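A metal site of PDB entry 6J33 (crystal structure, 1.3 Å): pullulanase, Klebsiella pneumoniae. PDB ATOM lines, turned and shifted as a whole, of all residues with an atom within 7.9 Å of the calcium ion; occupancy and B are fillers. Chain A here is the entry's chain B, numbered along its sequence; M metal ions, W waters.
Within 4 Å of the calcium ion: Ala 520, Asp 523, Tyr 525 and Asp 863.
The calcium ion is bound by OD1 of Asp 863 (2.3 Å), O of Tyr 525 (2.3 Å), water W1 (2.4 Å), water W2 (2.4 Å), OD1 of Asp 523 (2.4 Å), water W3 (2.5 Å) and O of Ala 520 (2.5 Å).
Water W1 lies within hydrogen-bond range of the backbone carbonyl oxygen of Asp 523 (2.8 Å) and the backbone carbonyl oxygen of Thr 454 (3.3 Å).
Water W2 bridges ND2 of Asn 526 and O of Thr 454.
Water W3 lies within hydrogen-bond range of the side-chain carboxylate of Asp 523 (2.7 Å), the backbone carbonyl oxygen of Asp 863 (2.9 Å) and the backbone NH of Gly 865 (3.4 Å).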
ATOM      1  N   THR A 454     -20.325  -3.741 -31.587  1.00  0.00           N
ATOM      2  CA  THR A 454     -20.065  -2.478 -30.891  1.00  0.00           C
ATOM      3  C   THR A 454     -18.598  -2.051 -30.851  1.00  0.00           C
ATOM      4  O   THR A 454     -18.238  -1.190 -30.043  1.00  0.00           O
ATOM      5  CB  THR A 454     -20.606  -2.580 -29.464  1.00  0.00           C
ATOM      6  OG1 THR A 454     -20.202  -3.830 -28.887  1.00  0.00           O
ATOM      7  CG2 THR A 454     -22.103  -2.468 -29.469  1.00  0.00           C
ATOM      8  N   VAL A 455     -17.751  -2.663 -31.662  1.00  0.00           N
ATOM      9  CA  VAL A 455     -16.410  -2.164 -31.937  1.00  0.00           C
ATOM     10  C   VAL A 455     -16.327  -2.000 -33.445  1.00  0.00           C
ATOM     11  O   VAL A 455     -16.759  -2.871 -34.199  1.00  0.00           O
ATOM     12  CB  VAL A 455     -15.337  -3.154 -31.442  1.00  0.00           C
ATOM     13  CG1 VAL A 455     -13.971  -2.753 -31.932  1.00  0.00           C
ATOM     14  CG2 VAL A 455     -15.353  -3.206 -29.918  1.00  0.00           C
ATOM     15  N   ASN A 456     -15.804  -0.858 -33.899  1.00  0.00           N
ATOM     16  CA  ASN A 456     -15.614  -0.642 -35.326  1.00  0.00           C
ATOM     17  C   ASN A 456     -14.363  -1.383 -35.760  1.00  0.00           C
ATOM     18  O   ASN A 456     -13.283  -1.141 -35.228  1.00  0.00           O
ATOM     19  CB  ASN A 456     -15.517   0.848 -35.639  1.00  0.00           C
ATOM     20  CG  ASN A 456     -15.697   1.128 -37.109  1.00  0.00           C
ATOM     21  OD1 ASN A 456     -15.182   0.398 -37.954  1.00  0.00           O
ATOM     22  ND2 ASN A 456     -16.443   2.172 -37.432  1.00  0.00           N
ATOM     23  N   ASP A 464      -7.226   4.149 -29.603  1.00  0.00           N
ATOM     24  CA  ASP A 464      -7.056   3.534 -28.297  1.00  0.00           C
ATOM     25  C   ASP A 464      -6.154   4.369 -27.404  1.00  0.00           C
ATOM     26  O   ASP A 464      -5.477   5.295 -27.865  1.00  0.00           O
ATOM     27  CB  ASP A 464      -6.552   2.096 -28.442  1.00  0.00           C
ATOM     28  CG  ASP A 464      -7.652   1.164 -28.893  1.00  0.00           C
ATOM     29  OD1 ASP A 464      -8.642   0.997 -28.132  1.00  0.00           O
ATOM     30  OD2 ASP A 464      -7.576   0.614 -30.015  1.00  0.00           O
ATOM     31  N   ASN A 516     -12.821   9.306 -20.143  1.00  0.00           N
ATOM     32  CA  ASN A 516     -12.868   7.916 -20.585  1.00  0.00           C
ATOM     33  C   ASN A 516     -14.207   7.562 -21.195  1.00  0.00           C
ATOM     34  O   ASN A 516     -14.263   6.719 -22.109  1.00  0.00           O
ATOM     35  CB  ASN A 516     -12.533   6.977 -19.440  1.00  0.00           C
ATOM     36  CG  ASN A 516     -12.152   5.605 -19.923  1.00  0.00           C
ATOM     37  OD1 ASN A 516     -11.224   5.465 -20.713  1.00  0.00           O
ATOM     38  ND2 ASN A 516     -12.858   4.587 -19.444  1.00  0.00           N
ATOM     39  N   THR A 517     -15.296   8.172 -20.712  1.00  0.00           N
ATOM     40  CA  THR A 517     -16.612   7.924 -21.284  1.00  0.00           C
ATOM     41  C   THR A 517     -16.663   8.328 -22.738  1.00  0.00           C
ATOM     42  O   THR A 517     -17.330   7.699 -23.558  1.00  0.00           O
ATOM     43  CB  THR A 517     -17.662   8.674 -20.465  1.00  0.00           C
ATOM     44  OG1 THR A 517     -17.684   8.163 -19.129  1.00  0.00           O
ATOM     45  CG2 THR A 517     -19.058   8.539 -21.094  1.00  0.00           C
ATOM     46  N   LEU A 518     -15.959   9.408 -23.086  1.00  0.00           N
ATOM     47  CA  LEU A 518     -15.894   9.820 -24.483  1.00  0.00           C
ATOM     48  C   LEU A 518     -15.016   8.867 -25.286  1.00  0.00           C
ATOM     49  O   LEU A 518     -15.371   8.468 -26.392  1.00  0.00           O
ATOM     50  CB  LEU A 518     -15.364  11.264 -24.584  1.00  0.00           C
ATOM     51  CG  LEU A 518     -16.199  12.292 -23.805  1.00  0.00           C
ATOM     52  CD1 LEU A 518     -15.597  13.679 -23.916  1.00  0.00           C
ATOM     53  CD2 LEU A 518     -17.658  12.284 -24.250  1.00  0.00           C
ATOM     54  N   VAL A 519     -13.852   8.494 -24.730  1.00  0.00           N
ATOM     55  CA  VAL A 519     -12.942   7.540 -25.359  1.00  0.00           C
ATOM     56  C   VAL A 519     -13.686   6.269 -25.747  1.00  0.00           C
ATOM     57  O   VAL A 519     -13.458   5.687 -26.825  1.00  0.00           O
ATOM     58  CB  VAL A 519     -11.773   7.229 -24.402  1.00  0.00           C
ATOM     59  CG1 VAL A 519     -10.947   6.042 -24.892  1.00  0.00           C
ATOM     60  CG2 VAL A 519     -10.907   8.442 -24.224  1.00  0.00           C
ATOM     61  N   ALA A 520     -14.599   5.818 -24.882  1.00  0.00           N
ATOM     62  CA  ALA A 520     -15.292   4.553 -25.075  1.00  0.00           C
ATOM     63  C   ALA A 520     -16.060   4.499 -26.384  1.00  0.00           C
ATOM     64  O   ALA A 520     -16.336   3.402 -26.877  1.00  0.00           O
ATOM     65  CB  ALA A 520     -16.277   4.358 -23.927  1.00  0.00           C
ATOM     66  N   GLN A 521     -16.447   5.652 -26.927  1.00  0.00           N
ATOM     67  CA  GLN A 521     -17.273   5.650 -28.135  1.00  0.00           C
ATOM     68  C   GLN A 521     -16.512   5.158 -29.344  1.00  0.00           C
ATOM     69  O   GLN A 521     -17.117   4.669 -30.305  1.00  0.00           O
ATOM     70  CB  GLN A 521     -17.783   7.059 -28.423  1.00  0.00           C
ATOM     71  CG  GLN A 521     -18.572   7.691 -27.299  1.00  0.00           C
ATOM     72  CD  GLN A 521     -18.948   9.119 -27.579  1.00  0.00           C
ATOM     73  OE1 GLN A 521     -18.738   9.627 -28.688  1.00  0.00           O
ATOM     74  NE2 GLN A 521     -19.521   9.788 -26.592  1.00  0.00           N
ATOM     75  N   THR A 522     -15.192   5.290 -29.345  1.00  0.00           N
ATOM     76  CA  THR A 522     -14.384   5.057 -30.538  1.00  0.00           C
ATOM     77  C   THR A 522     -13.173   4.187 -30.267  1.00  0.00           C
ATOM     78  O   THR A 522     -12.256   4.153 -31.090  1.00  0.00           O
ATOM     79  CB  THR A 522     -13.993   6.374 -31.237  1.00  0.00           C
ATOM     80  OG1 THR A 522     -13.345   7.251 -30.307  1.00  0.00           O
ATOM     81  CG2 THR A 522     -15.211   7.087 -31.800  1.00  0.00           C
ATOM     82  N   ASP A 523     -13.127   3.492 -29.121  1.00  0.00           N
ATOM     83  CA  ASP A 523     -11.992   2.626 -28.845  1.00  0.00           C
ATOM     84  C   ASP A 523     -12.264   1.198 -29.316  1.00  0.00           C
ATOM     85  O   ASP A 523     -13.281   0.887 -29.933  1.00  0.00           O
ATOM     86  CB  ASP A 523     -11.595   2.703 -27.362  1.00  0.00           C
ATOM     87  CG  ASP A 523     -12.664   2.127 -26.408  1.00  0.00           C
ATOM     88  OD1 ASP A 523     -13.620   1.483 -26.881  1.00  0.00           O
ATOM     89  OD2 ASP A 523     -12.523   2.303 -25.163  1.00  0.00           O
ATOM     90  N   SER A 524     -11.320   0.302 -29.026  1.00  0.00           N
ATOM     91  CA  SER A 524     -11.407  -1.110 -29.389  1.00  0.00           C
ATOM     92  C   SER A 524     -12.132  -1.965 -28.355  1.00  0.00           C
ATOM     93  O   SER A 524     -12.177  -3.186 -28.501  1.00  0.00           O
ATOM     94  CB  SER A 524     -10.021  -1.693 -29.622  1.00  0.00           C
ATOM     95  OG  SER A 524      -9.386  -1.073 -30.725  1.00  0.00           O
ATOM     96  N   TYR A 525     -12.683  -1.372 -27.297  1.00  0.00           N
ATOM     97  CA  TYR A 525     -13.097  -2.103 -26.113  1.00  0.00           C
ATOM     98  C   TYR A 525     -14.599  -2.279 -26.019  1.00  0.00           C
ATOM     99  O   TYR A 525     -15.348  -1.301 -26.017  1.00  0.00           O
ATOM    100  CB  TYR A 525     -12.600  -1.430 -24.825  1.00  0.00           C
ATOM    101  CG  TYR A 525     -12.709  -2.381 -23.677  1.00  0.00           C
ATOM    102  CD1 TYR A 525     -13.920  -2.592 -23.019  1.00  0.00           C
ATOM    103  CD2 TYR A 525     -11.623  -3.151 -23.310  1.00  0.00           C
ATOM    104  CE1 TYR A 525     -14.046  -3.520 -22.020  1.00  0.00           C
ATOM    105  CE2 TYR A 525     -11.739  -4.091 -22.283  1.00  0.00           C
ATOM    106  CZ  TYR A 525     -12.957  -4.276 -21.670  1.00  0.00           C
ATOM    107  OH  TYR A 525     -13.092  -5.200 -20.669  1.00  0.00           O
ATOM    108  N   ASN A 526     -15.053  -3.530 -25.880  1.00  0.00           N
ATOM    109  CA  ASN A 526     -16.404  -3.816 -25.421  1.00  0.00           C
ATOM    110  C   ASN A 526     -16.418  -5.277 -24.981  1.00  0.00           C
ATOM    111  O   ASN A 526     -15.713  -6.110 -25.574  1.00  0.00           O
ATOM    112  CB  ASN A 526     -17.437  -3.627 -26.543  1.00  0.00           C
ATOM    113  CG  ASN A 526     -18.842  -3.443 -26.004  1.00  0.00           C
ATOM    114  OD1 ASN A 526     -19.474  -4.389 -25.552  1.00  0.00           O
ATOM    115  ND2 ASN A 526     -19.339  -2.211 -26.020  1.00  0.00           N
ATOM    116  N   TRP A 527     -17.188  -5.594 -23.931  1.00  0.00           N
ATOM    117  CA  TRP A 527     -17.393  -7.007 -23.612  1.00  0.00           C
ATOM    118  C   TRP A 527     -17.915  -7.767 -24.818  1.00  0.00           C
ATOM    119  O   TRP A 527     -17.553  -8.929 -25.035  1.00  0.00           O
ATOM    120  CB  TRP A 527     -18.388  -7.194 -22.472  1.00  0.00           C
ATOM    121  CG  TRP A 527     -17.890  -6.869 -21.134  1.00  0.00           C
ATOM    122  CD1 TRP A 527     -16.608  -6.659 -20.758  1.00  0.00           C
ATOM    123  CD2 TRP A 527     -18.695  -6.708 -19.982  1.00  0.00           C
ATOM    124  NE1 TRP A 527     -16.560  -6.371 -19.393  1.00  0.00           N
ATOM    125  CE2 TRP A 527     -17.841  -6.354 -18.907  1.00  0.00           C
ATOM    126  CE3 TRP A 527     -20.070  -6.765 -19.750  1.00  0.00           C
ATOM    127  CZ2 TRP A 527     -18.312  -6.134 -17.624  1.00  0.00           C
ATOM    128  CZ3 TRP A 527     -20.543  -6.518 -18.480  1.00  0.00           C
ATOM    129  CH2 TRP A 527     -19.663  -6.193 -17.435  1.00  0.00           C
ATOM    130  N   TYR A 862     -18.641  -2.895 -19.040  1.00  0.00           N
ATOM    131  CA  TYR A 862     -18.687  -3.412 -20.416  1.00  0.00           C
ATOM    132  C   TYR A 862     -18.101  -2.451 -21.443  1.00  0.00           C
ATOM    133  O   TYR A 862     -17.628  -2.898 -22.509  1.00  0.00           O
ATOM    134  CB  TYR A 862     -20.144  -3.723 -20.809  1.00  0.00           C
ATOM    135  CG  TYR A 862     -21.001  -2.524 -21.104  1.00  0.00           C
ATOM    136  CD1 TYR A 862     -21.498  -1.732 -20.077  1.00  0.00           C
ATOM    137  CD2 TYR A 862     -21.334  -2.184 -22.403  1.00  0.00           C
ATOM    138  CE1 TYR A 862     -22.294  -0.631 -20.339  1.00  0.00           C
ATOM    139  CE2 TYR A 862     -22.136  -1.088 -22.677  1.00  0.00           C
ATOM    140  CZ  TYR A 862     -22.605  -0.312 -21.646  1.00  0.00           C
ATOM    141  OH  TYR A 862     -23.392   0.786 -21.910  1.00  0.00           O
ATOM    142  N   ASP A 863     -18.167  -1.129 -21.190  1.00  0.00           N
ATOM    143  CA  ASP A 863     -17.693  -0.110 -22.122  1.00  0.00           C
ATOM    144  C   ASP A 863     -16.744   0.850 -21.415  1.00  0.00           C
ATOM    145  O   ASP A 863     -16.549   1.969 -21.877  1.00  0.00           O
ATOM    146  CB  ASP A 863     -18.896   0.632 -22.739  1.00  0.00           C
ATOM    147  CG  ASP A 863     -18.585   1.264 -24.101  1.00  0.00           C
ATOM    148  OD1 ASP A 863     -17.533   0.981 -24.709  1.00  0.00           O
ATOM    149  OD2 ASP A 863     -19.434   2.071 -24.555  1.00  0.00           O
ATOM    150  N   SER A 864     -16.143   0.414 -20.293  1.00  0.00           N
ATOM    151  CA  SER A 864     -15.255   1.255 -19.491  1.00  0.00           C
ATOM    152  C   SER A 864     -13.801   1.161 -19.936  1.00  0.00           C
ATOM    153  O   SER A 864     -12.913   1.722 -19.263  1.00  0.00           O
ATOM    154  CB  SER A 864     -15.409   0.969 -17.992  1.00  0.00           C
ATOM    155  OG  SER A 864     -16.664   1.429 -17.531  1.00  0.00           O
ATOM    156  N   GLY A 865     -13.549   0.507 -21.056  1.00  0.00           N
ATOM    157  CA  GLY A 865     -12.271   0.630 -21.732  1.00  0.00           C
ATOM    158  C   GLY A 865     -11.134  -0.139 -21.097  1.00  0.00           C
ATOM    159  O   GLY A 865     -11.263  -0.836 -20.097  1.00  0.00           O
ATOM    160  N   ASP A 866      -9.972   0.012 -21.737  1.00  0.00           N
ATOM    161  CA  ASP A 866      -8.735  -0.531 -21.202  1.00  0.00           C
ATOM    162  C   ASP A 866      -8.412   0.049 -19.826  1.00  0.00           C
ATOM    163  O   ASP A 866      -7.803  -0.632 -19.000  1.00  0.00           O
ATOM    164  CB  ASP A 866      -7.559  -0.213 -22.130  1.00  0.00           C
ATOM    165  CG  ASP A 866      -7.591  -0.981 -23.451  1.00  0.00           C
ATOM    166  OD1 ASP A 866      -8.226  -2.045 -23.550  1.00  0.00           O
ATOM    167  OD2 ASP A 866      -6.900  -0.503 -24.379  1.00  0.00           O
HETATM  168 CA    CA M   1     -15.924   0.943 -26.373  1.00  0.00          CA
HETATM  169  O   HOH W   1     -15.776   0.629 -28.712  1.00  0.00           O
HETATM  170  O   HOH W   2     -18.045   0.183 -27.246  1.00  0.00           O
HETATM  171  O   HOH W   3     -14.841   1.258 -24.117  1.00  0.00           O
